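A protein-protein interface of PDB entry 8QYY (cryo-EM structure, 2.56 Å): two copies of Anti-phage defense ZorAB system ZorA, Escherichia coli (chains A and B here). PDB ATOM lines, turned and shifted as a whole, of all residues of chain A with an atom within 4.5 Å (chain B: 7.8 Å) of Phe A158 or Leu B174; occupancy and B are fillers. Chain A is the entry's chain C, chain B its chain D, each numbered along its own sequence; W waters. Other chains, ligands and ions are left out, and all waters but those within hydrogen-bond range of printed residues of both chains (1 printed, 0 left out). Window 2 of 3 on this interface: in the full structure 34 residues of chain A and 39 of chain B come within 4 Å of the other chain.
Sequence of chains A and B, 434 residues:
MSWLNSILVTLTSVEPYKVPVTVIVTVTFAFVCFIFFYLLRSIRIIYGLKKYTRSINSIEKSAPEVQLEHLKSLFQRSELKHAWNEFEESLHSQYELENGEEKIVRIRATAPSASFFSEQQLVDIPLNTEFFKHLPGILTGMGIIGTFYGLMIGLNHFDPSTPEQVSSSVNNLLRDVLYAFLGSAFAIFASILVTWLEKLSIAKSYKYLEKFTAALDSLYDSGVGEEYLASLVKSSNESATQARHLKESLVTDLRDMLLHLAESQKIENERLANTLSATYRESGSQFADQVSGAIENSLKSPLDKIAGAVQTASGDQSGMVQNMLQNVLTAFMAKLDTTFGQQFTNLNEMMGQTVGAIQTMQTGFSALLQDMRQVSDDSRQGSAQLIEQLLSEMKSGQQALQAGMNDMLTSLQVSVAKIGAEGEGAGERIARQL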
ATOM      1  N   GLY A 154       6.760 -16.196   5.735  1.00  0.00           N
ATOM      2  CA  GLY A 154       5.897 -17.325   6.052  1.00  0.00           C
ATOM      3  C   GLY A 154       4.973 -17.710   4.911  1.00  0.00           C
ATOM      4  O   GLY A 154       4.760 -18.895   4.646  1.00  0.00           O
ATOM      5  N   LEU A 155       4.408 -16.716   4.227  1.00  0.00           N
ATOM      6  CA  LEU A 155       3.430 -16.984   3.178  1.00  0.00           C
ATOM      7  C   LEU A 155       4.096 -17.513   1.914  1.00  0.00           C
ATOM      8  O   LEU A 155       3.563 -18.417   1.262  1.00  0.00           O
ATOM      9  CB  LEU A 155       2.637 -15.717   2.870  1.00  0.00           C
ATOM     10  CG  LEU A 155       1.725 -15.166   3.966  1.00  0.00           C
ATOM     11  CD1 LEU A 155       1.531 -13.674   3.791  1.00  0.00           C
ATOM     12  CD2 LEU A 155       0.394 -15.873   3.968  1.00  0.00           C
ATOM     13  N   ASN A 156       5.250 -16.956   1.544  1.00  0.00           N
ATOM     14  CA  ASN A 156       5.897 -17.374   0.304  1.00  0.00           C
ATOM     15  C   ASN A 156       6.379 -18.816   0.387  1.00  0.00           C
ATOM     16  O   ASN A 156       6.362 -19.541  -0.613  1.00  0.00           O
ATOM     17  CB  ASN A 156       7.057 -16.439  -0.029  1.00  0.00           C
ATOM     18  CG  ASN A 156       7.510 -16.569  -1.468  1.00  0.00           C
ATOM     19  OD1 ASN A 156       6.736 -16.951  -2.341  1.00  0.00           O
ATOM     20  ND2 ASN A 156       8.773 -16.256  -1.721  1.00  0.00           N
ATOM     21  N   HIS A 157       6.812 -19.251   1.567  1.00  0.00           N
ATOM     22  CA  HIS A 157       7.316 -20.602   1.763  1.00  0.00           C
ATOM     23  C   HIS A 157       6.226 -21.592   2.144  1.00  0.00           C
ATOM     24  O   HIS A 157       6.539 -22.693   2.610  1.00  0.00           O
ATOM     25  CB  HIS A 157       8.420 -20.605   2.821  1.00  0.00           C
ATOM     26  CG  HIS A 157       9.727 -20.069   2.328  1.00  0.00           C
ATOM     27  ND1 HIS A 157      10.084 -20.092   0.999  1.00  0.00           N
ATOM     28  CD2 HIS A 157      10.764 -19.501   2.987  1.00  0.00           C
ATOM     29  CE1 HIS A 157      11.285 -19.561   0.859  1.00  0.00           C
ATOM     30  NE2 HIS A 157      11.720 -19.194   2.051  1.00  0.00           N
ATOM     31  N   PHE A 158       4.960 -21.233   1.964  1.00  0.00           N
ATOM     32  CA  PHE A 158       3.878 -22.170   2.233  1.00  0.00           C
ATOM     33  C   PHE A 158       3.867 -23.261   1.171  1.00  0.00           C
ATOM     34  O   PHE A 158       3.824 -22.975  -0.029  1.00  0.00           O
ATOM     35  CB  PHE A 158       2.537 -21.443   2.266  1.00  0.00           C
ATOM     36  CG  PHE A 158       1.384 -22.314   2.674  1.00  0.00           C
ATOM     37  CD1 PHE A 158       1.124 -22.562   4.008  1.00  0.00           C
ATOM     38  CD2 PHE A 158       0.553 -22.874   1.721  1.00  0.00           C
ATOM     39  CE1 PHE A 158       0.067 -23.356   4.385  1.00  0.00           C
ATOM     40  CE2 PHE A 158      -0.508 -23.670   2.093  1.00  0.00           C
ATOM     41  CZ  PHE A 158      -0.752 -23.911   3.428  1.00  0.00           C
ATOM     42  N   ASP A 159       3.903 -24.512   1.616  1.00  0.00           N
ATOM     43  CA  ASP A 159       4.002 -25.666   0.723  1.00  0.00           C
ATOM     44  C   ASP A 159       2.788 -26.563   0.917  1.00  0.00           C
ATOM     45  O   ASP A 159       2.754 -27.373   1.859  1.00  0.00           O
ATOM     46  CB  ASP A 159       5.295 -26.435   0.990  1.00  0.00           C
ATOM     47  CG  ASP A 159       5.504 -27.580   0.026  1.00  0.00           C
ATOM     48  OD1 ASP A 159       4.851 -27.600  -1.037  1.00  0.00           O
ATOM     49  OD2 ASP A 159       6.333 -28.462   0.332  1.00  0.00           O
ATOM     50  N   PRO A 160       1.769 -26.453   0.067  1.00  0.00           N
ATOM     51  CA  PRO A 160       0.555 -27.267   0.220  1.00  0.00           C
ATOM     52  C   PRO A 160       0.585 -28.611  -0.492  1.00  0.00           C
ATOM     53  O   PRO A 160      -0.474 -29.230  -0.633  1.00  0.00           O
ATOM     54  CB  PRO A 160      -0.510 -26.365  -0.407  1.00  0.00           C
ATOM     55  CG  PRO A 160       0.223 -25.677  -1.512  1.00  0.00           C
ATOM     56  CD  PRO A 160       1.659 -25.516  -1.062  1.00  0.00           C
ATOM     57  N   SER A 169       4.228 -26.117   7.162  1.00  0.00           N
ATOM     58  CA  SER A 169       4.027 -24.749   6.699  1.00  0.00           C
ATOM     59  C   SER A 169       3.140 -23.964   7.656  1.00  0.00           C
ATOM     60  O   SER A 169       3.381 -22.779   7.911  1.00  0.00           O
ATOM     61  CB  SER A 169       3.426 -24.763   5.295  1.00  0.00           C
ATOM     62  OG  SER A 169       4.256 -25.469   4.392  1.00  0.00           O
ATOM     63  N   VAL A 170       2.108 -24.611   8.197  1.00  0.00           N
ATOM     64  CA  VAL A 170       1.234 -23.952   9.162  1.00  0.00           C
ATOM     65  C   VAL A 170       1.988 -23.654  10.453  1.00  0.00           C
ATOM     66  O   VAL A 170       1.820 -22.586  11.057  1.00  0.00           O
ATOM     67  CB  VAL A 170      -0.016 -24.814   9.411  1.00  0.00           C
ATOM     68  CG1 VAL A 170      -0.730 -24.368  10.663  1.00  0.00           C
ATOM     69  CG2 VAL A 170      -0.943 -24.750   8.215  1.00  0.00           C
ATOM     70  N   LEU A 173       4.038 -20.670   9.801  1.00  0.00           N
ATOM     71  CA  LEU A 173       3.207 -19.467   9.813  1.00  0.00           C
ATOM     72  C   LEU A 173       2.902 -19.017  11.236  1.00  0.00           C
ATOM     73  O   LEU A 173       2.950 -17.821  11.542  1.00  0.00           O
ATOM     74  CB  LEU A 173       1.912 -19.715   9.044  1.00  0.00           C
ATOM     75  CG  LEU A 173       1.853 -19.163   7.621  1.00  0.00           C
ATOM     76  CD1 LEU A 173       0.527 -19.505   6.981  1.00  0.00           C
ATOM     77  CD2 LEU A 173       2.074 -17.665   7.626  1.00  0.00           C
ATOM     78  N   GLY B 154      -8.111 -10.984  -2.471  1.00  0.00           N
ATOM     79  CA  GLY B 154      -7.852 -12.306  -1.926  1.00  0.00           C
ATOM     80  C   GLY B 154      -9.067 -12.920  -1.262  1.00  0.00           C
ATOM     81  O   GLY B 154      -9.333 -14.113  -1.420  1.00  0.00           O
ATOM     82  N   PHE B 158     -11.448 -16.213  -2.327  1.00  0.00           N
ATOM     83  CA  PHE B 158     -11.442 -17.304  -1.357  1.00  0.00           C
ATOM     84  C   PHE B 158     -12.874 -17.744  -1.079  1.00  0.00           C
ATOM     85  O   PHE B 158     -13.645 -17.014  -0.451  1.00  0.00           O
ATOM     86  CB  PHE B 158     -10.743 -16.867  -0.074  1.00  0.00           C
ATOM     87  CG  PHE B 158     -10.772 -17.897   1.017  1.00  0.00           C
ATOM     88  CD1 PHE B 158      -9.879 -18.950   1.017  1.00  0.00           C
ATOM     89  CD2 PHE B 158     -11.684 -17.804   2.049  1.00  0.00           C
ATOM     90  CE1 PHE B 158      -9.903 -19.894   2.018  1.00  0.00           C
ATOM     91  CE2 PHE B 158     -11.710 -18.744   3.052  1.00  0.00           C
ATOM     92  CZ  PHE B 158     -10.818 -19.790   3.035  1.00  0.00           C
ATOM     93  N   VAL B 166     -10.676 -26.841   0.170  1.00  0.00           N
ATOM     94  CA  VAL B 166     -10.115 -25.982   1.205  1.00  0.00           C
ATOM     95  C   VAL B 166      -8.634 -25.728   0.949  1.00  0.00           C
ATOM     96  O   VAL B 166      -8.148 -24.605   1.119  1.00  0.00           O
ATOM     97  CB  VAL B 166     -10.361 -26.597   2.594  1.00  0.00           C
ATOM     98  CG1 VAL B 166      -9.467 -25.951   3.631  1.00  0.00           C
ATOM     99  CG2 VAL B 166     -11.818 -26.446   2.982  1.00  0.00           C
ATOM    100  N   SER B 167      -7.896 -26.759   0.533  1.00  0.00           N
ATOM    101  CA  SER B 167      -6.452 -26.627   0.369  1.00  0.00           C
ATOM    102  C   SER B 167      -6.099 -25.610  -0.713  1.00  0.00           C
ATOM    103  O   SER B 167      -5.256 -24.727  -0.505  1.00  0.00           O
ATOM    104  CB  SER B 167      -5.842 -27.992   0.049  1.00  0.00           C
ATOM    105  OG  SER B 167      -4.428 -27.932   0.025  1.00  0.00           O
ATOM    106  N   SER B 168      -6.733 -25.722  -1.883  1.00  0.00           N
ATOM    107  CA  SER B 168      -6.441 -24.802  -2.978  1.00  0.00           C
ATOM    108  C   SER B 168      -6.852 -23.378  -2.631  1.00  0.00           C
ATOM    109  O   SER B 168      -6.135 -22.421  -2.950  1.00  0.00           O
ATOM    110  CB  SER B 168      -7.147 -25.265  -4.249  1.00  0.00           C
ATOM    111  OG  SER B 168      -6.653 -26.521  -4.677  1.00  0.00           O
ATOM    112  N   SER B 169      -8.013 -23.219  -1.992  1.00  0.00           N
ATOM    113  CA  SER B 169      -8.460 -21.895  -1.582  1.00  0.00           C
ATOM    114  C   SER B 169      -7.481 -21.271  -0.598  1.00  0.00           C
ATOM    115  O   SER B 169      -7.149 -20.088  -0.709  1.00  0.00           O
ATOM    116  CB  SER B 169      -9.854 -21.984  -0.966  1.00  0.00           C
ATOM    117  OG  SER B 169     -10.765 -22.595  -1.856  1.00  0.00           O
ATOM    118  N   VAL B 170      -7.000 -22.061   0.364  1.00  0.00           N
ATOM    119  CA  VAL B 170      -6.041 -21.556   1.339  1.00  0.00           C
ATOM    120  C   VAL B 170      -4.749 -21.140   0.648  1.00  0.00           C
ATOM    121  O   VAL B 170      -4.186 -20.080   0.942  1.00  0.00           O
ATOM    122  CB  VAL B 170      -5.792 -22.613   2.430  1.00  0.00           C
ATOM    123  CG1 VAL B 170      -4.502 -22.322   3.172  1.00  0.00           C
ATOM    124  CG2 VAL B 170      -6.960 -22.657   3.395  1.00  0.00           C
ATOM    125  N   ASN B 171      -4.267 -21.959  -0.289  1.00  0.00           N
ATOM    126  CA  ASN B 171      -3.025 -21.636  -0.985  1.00  0.00           C
ATOM    127  C   ASN B 171      -3.151 -20.339  -1.779  1.00  0.00           C
ATOM    128  O   ASN B 171      -2.284 -19.453  -1.699  1.00  0.00           O
ATOM    129  CB  ASN B 171      -2.632 -22.799  -1.897  1.00  0.00           C
ATOM    130  CG  ASN B 171      -1.345 -22.544  -2.646  1.00  0.00           C
ATOM    131  OD1 ASN B 171      -0.260 -22.577  -2.069  1.00  0.00           O
ATOM    132  ND2 ASN B 171      -1.456 -22.297  -3.945  1.00  0.00           N
ATOM    133  N   ASN B 172      -4.234 -20.199  -2.546  1.00  0.00           N
ATOM    134  CA  ASN B 172      -4.417 -18.992  -3.343  1.00  0.00           C
ATOM    135  C   ASN B 172      -4.606 -17.765  -2.458  1.00  0.00           C
ATOM    136  O   ASN B 172      -4.090 -16.679  -2.767  1.00  0.00           O
ATOM    137  CB  ASN B 172      -5.600 -19.167  -4.289  1.00  0.00           C
ATOM    138  CG  ASN B 172      -5.388 -20.293  -5.279  1.00  0.00           C
ATOM    139  OD1 ASN B 172      -4.258 -20.708  -5.530  1.00  0.00           O
ATOM    140  ND2 ASN B 172      -6.475 -20.787  -5.851  1.00  0.00           N
ATOM    141  N   LEU B 173      -5.333 -17.917  -1.351  1.00  0.00           N
ATOM    142  CA  LEU B 173      -5.502 -16.811  -0.419  1.00  0.00           C
ATOM    143  C   LEU B 173      -4.168 -16.379   0.165  1.00  0.00           C
ATOM    144  O   LEU B 173      -3.912 -15.179   0.321  1.00  0.00           O
ATOM    145  CB  LEU B 173      -6.463 -17.211   0.695  1.00  0.00           C
ATOM    146  CG  LEU B 173      -6.610 -16.211   1.836  1.00  0.00           C
ATOM    147  CD1 LEU B 173      -7.267 -14.931   1.359  1.00  0.00           C
ATOM    148  CD2 LEU B 173      -7.397 -16.840   2.947  1.00  0.00           C
ATOM    149  N   LEU B 174      -3.309 -17.337   0.511  1.00  0.00           N
ATOM    150  CA  LEU B 174      -2.002 -16.983   1.049  1.00  0.00           C
ATOM    151  C   LEU B 174      -1.158 -16.261   0.011  1.00  0.00           C
ATOM    152  O   LEU B 174      -0.423 -15.328   0.346  1.00  0.00           O
ATOM    153  CB  LEU B 174      -1.280 -18.226   1.562  1.00  0.00           C
ATOM    154  CG  LEU B 174      -1.921 -18.915   2.764  1.00  0.00           C
ATOM    155  CD1 LEU B 174      -0.899 -19.761   3.479  1.00  0.00           C
ATOM    156  CD2 LEU B 174      -2.543 -17.905   3.709  1.00  0.00           C
ATOM    157  N   ARG B 175      -1.254 -16.665  -1.257  1.00  0.00           N
ATOM    158  CA  ARG B 175      -0.528 -15.948  -2.304  1.00  0.00           C
ATOM    159  C   ARG B 175      -1.003 -14.499  -2.421  1.00  0.00           C
ATOM    160  O   ARG B 175      -0.189 -13.565  -2.512  1.00  0.00           O
ATOM    161  CB  ARG B 175      -0.684 -16.680  -3.635  1.00  0.00           C
ATOM    162  CG  ARG B 175      -0.100 -15.950  -4.828  1.00  0.00           C
ATOM    163  CD  ARG B 175       1.395 -15.728  -4.680  1.00  0.00           C
ATOM    164  NE  ARG B 175       2.086 -16.911  -4.183  1.00  0.00           N
ATOM    165  CZ  ARG B 175       3.383 -17.135  -4.335  1.00  0.00           C
ATOM    166  NH1 ARG B 175       4.158 -16.286  -4.989  1.00  0.00           N
ATOM    167  NH2 ARG B 175       3.916 -18.238  -3.818  1.00  0.00           N
ATOM    168  N   ASP B 176      -2.322 -14.291  -2.408  1.00  0.00           N
ATOM    169  CA  ASP B 176      -2.854 -12.934  -2.508  1.00  0.00           C
ATOM    170  C   ASP B 176      -2.463 -12.087  -1.298  1.00  0.00           C
ATOM    171  O   ASP B 176      -2.111 -10.904  -1.439  1.00  0.00           O
ATOM    172  CB  ASP B 176      -4.370 -12.988  -2.665  1.00  0.00           C
ATOM    173  CG  ASP B 176      -4.796 -13.682  -3.941  1.00  0.00           C
ATOM    174  OD1 ASP B 176      -3.971 -13.761  -4.874  1.00  0.00           O
ATOM    175  OD2 ASP B 176      -5.950 -14.149  -4.016  1.00  0.00           O
ATOM    176  N   VAL B 177      -2.519 -12.676  -0.102  1.00  0.00           N
ATOM    177  CA  VAL B 177      -2.095 -11.968   1.101  1.00  0.00           C
ATOM    178  C   VAL B 177      -0.616 -11.622   1.020  1.00  0.00           C
ATOM    179  O   VAL B 177      -0.188 -10.553   1.470  1.00  0.00           O
ATOM    180  CB  VAL B 177      -2.416 -12.803   2.354  1.00  0.00           C
ATOM    181  CG1 VAL B 177      -1.780 -12.179   3.575  1.00  0.00           C
ATOM    182  CG2 VAL B 177      -3.911 -12.909   2.542  1.00  0.00           C
ATOM    183  N   LEU B 178       0.189 -12.519   0.450  1.00  0.00           N
ATOM    184  CA  LEU B 178       1.608 -12.236   0.275  1.00  0.00           C
ATOM    185  C   LEU B 178       1.819 -11.019  -0.609  1.00  0.00           C
ATOM    186  O   LEU B 178       2.663 -10.166  -0.314  1.00  0.00           O
ATOM    187  CB  LEU B 178       2.312 -13.457  -0.318  1.00  0.00           C
ATOM    188  CG  LEU B 178       3.668 -13.232  -0.985  1.00  0.00           C
ATOM    189  CD1 LEU B 178       4.739 -12.950   0.051  1.00  0.00           C
ATOM    190  CD2 LEU B 178       4.042 -14.427  -1.830  1.00  0.00           C
ATOM    191  N   TYR B 179       1.058 -10.918  -1.701  1.00  0.00           N
ATOM    192  CA  TYR B 179       1.186  -9.751  -2.573  1.00  0.00           C
ATOM    193  C   TYR B 179       0.811  -8.463  -1.840  1.00  0.00           C
ATOM    194  O   TYR B 179       1.527  -7.449  -1.914  1.00  0.00           O
ATOM    195  CB  TYR B 179       0.321  -9.937  -3.816  1.00  0.00           C
ATOM    196  CG  TYR B 179       0.889 -10.921  -4.805  1.00  0.00           C
ATOM    197  CD1 TYR B 179       2.254 -11.005  -5.020  1.00  0.00           C
ATOM    198  CD2 TYR B 179       0.060 -11.773  -5.516  1.00  0.00           C
ATOM    199  CE1 TYR B 179       2.777 -11.905  -5.918  1.00  0.00           C
ATOM    200  CE2 TYR B 179       0.577 -12.676  -6.416  1.00  0.00           C
ATOM    201  CZ  TYR B 179       1.936 -12.739  -6.612  1.00  0.00           C
ATOM    202  OH  TYR B 179       2.454 -13.638  -7.513  1.00  0.00           O
ATOM    203  N   ALA B 180      -0.307  -8.491  -1.111  1.00  0.00           N
ATOM    204  CA  ALA B 180      -0.731  -7.300  -0.374  1.00  0.00           C
ATOM    205  C   ALA B 180       0.309  -6.891   0.665  1.00  0.00           C
ATOM    206  O   ALA B 180       0.616  -5.698   0.825  1.00  0.00           O
ATOM    207  CB  ALA B 180      -2.083  -7.548   0.288  1.00  0.00           C
ATOM    208  N   PHE B 181       0.868  -7.872   1.375  1.00  0.00           N
ATOM    209  CA  PHE B 181       1.868  -7.582   2.394  1.00  0.00           C
ATOM    210  C   PHE B 181       3.143  -7.037   1.773  1.00  0.00           C
ATOM    211  O   PHE B 181       3.800  -6.176   2.361  1.00  0.00           O
ATOM    212  CB  PHE B 181       2.167  -8.835   3.210  1.00  0.00           C
ATOM    213  CG  PHE B 181       1.117  -9.164   4.224  1.00  0.00           C
ATOM    214  CD1 PHE B 181      -0.127  -8.563   4.172  1.00  0.00           C
ATOM    215  CD2 PHE B 181       1.375 -10.066   5.235  1.00  0.00           C
ATOM    216  CE1 PHE B 181      -1.091  -8.863   5.099  1.00  0.00           C
ATOM    217  CE2 PHE B 181       0.411 -10.368   6.169  1.00  0.00           C
ATOM    218  CZ  PHE B 181      -0.822  -9.765   6.101  1.00  0.00           C
HETATM  219  O   HOH W   1       2.151 -18.018  -0.855  1.00  0.00           O
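Of chain B, only Asn B171 (3.9 Å) and Leu B174 (3.5 Å) come within 4 Å of Phe A158. Of the printed residues of chain A, Asn B171 touches Phe A158 and Pro A160. Of the printed residues of chain B, Leu A155 touches Leu B174, Val B177, Leu B178 and Phe B181. Ser A169 touches none of the printed residues of chain B. Val B170 touches none of the printed residues of chain A. The nearest residue of chain B that does not touch Phe A158 is Val B170 (4.1 Å). The nearest printed residue of chain A that does not touch Leu B174 is Gly A154 (5.8 Å). The nearest printed residue of chain B that does not touch Asn A156 is Leu B174 (6.0 Å).
The guanidinium group of Arg B175 is in hydrogen-bond range of the side-chain amide oxygen of Asn A156.
Positions printed for both chains: 154, 158, 169, 170 and 173. Of the 10 pairs that touch across the chains among the printed residues, none has its exchanged pair printed and touching as well.
Water W1 lies within hydrogen-bond range of O of Leu A155 and NH2 of Arg B175.
Among the printed residues, pairs that only touch across the chains: Pro A160 with Asn B171, Phe A158 with Leu B174, Leu A155 with Leu B174, Leu A155 with Val B177, Asn A156 with Leu B178, Leu A155 with Leu B178, Leu A173 with Leu B174, Phe A158 with Asn B171 and Leu A155 with Phe B181.
Of the 18 printed residues of chain B, 6 touch a printed residue of chain A. Hydrophobic or aromatic side chains of chain B that line the printed part of chain A: Leu B174, Val B177, Leu B178 and Phe B181. Along chain B the printed residues that touch a printed residue of chain A span positions 171 to 181. Of the 10 printed residues of chain A, 5 touch a printed residue of chain B. Hydrophobic or aromatic side chains of chain A within 4 Å of the printed part of chain B: Leu A155, Phe A158, Pro A160 and Leu A173. Among the printed residues, 10 pairs touch across the chains.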
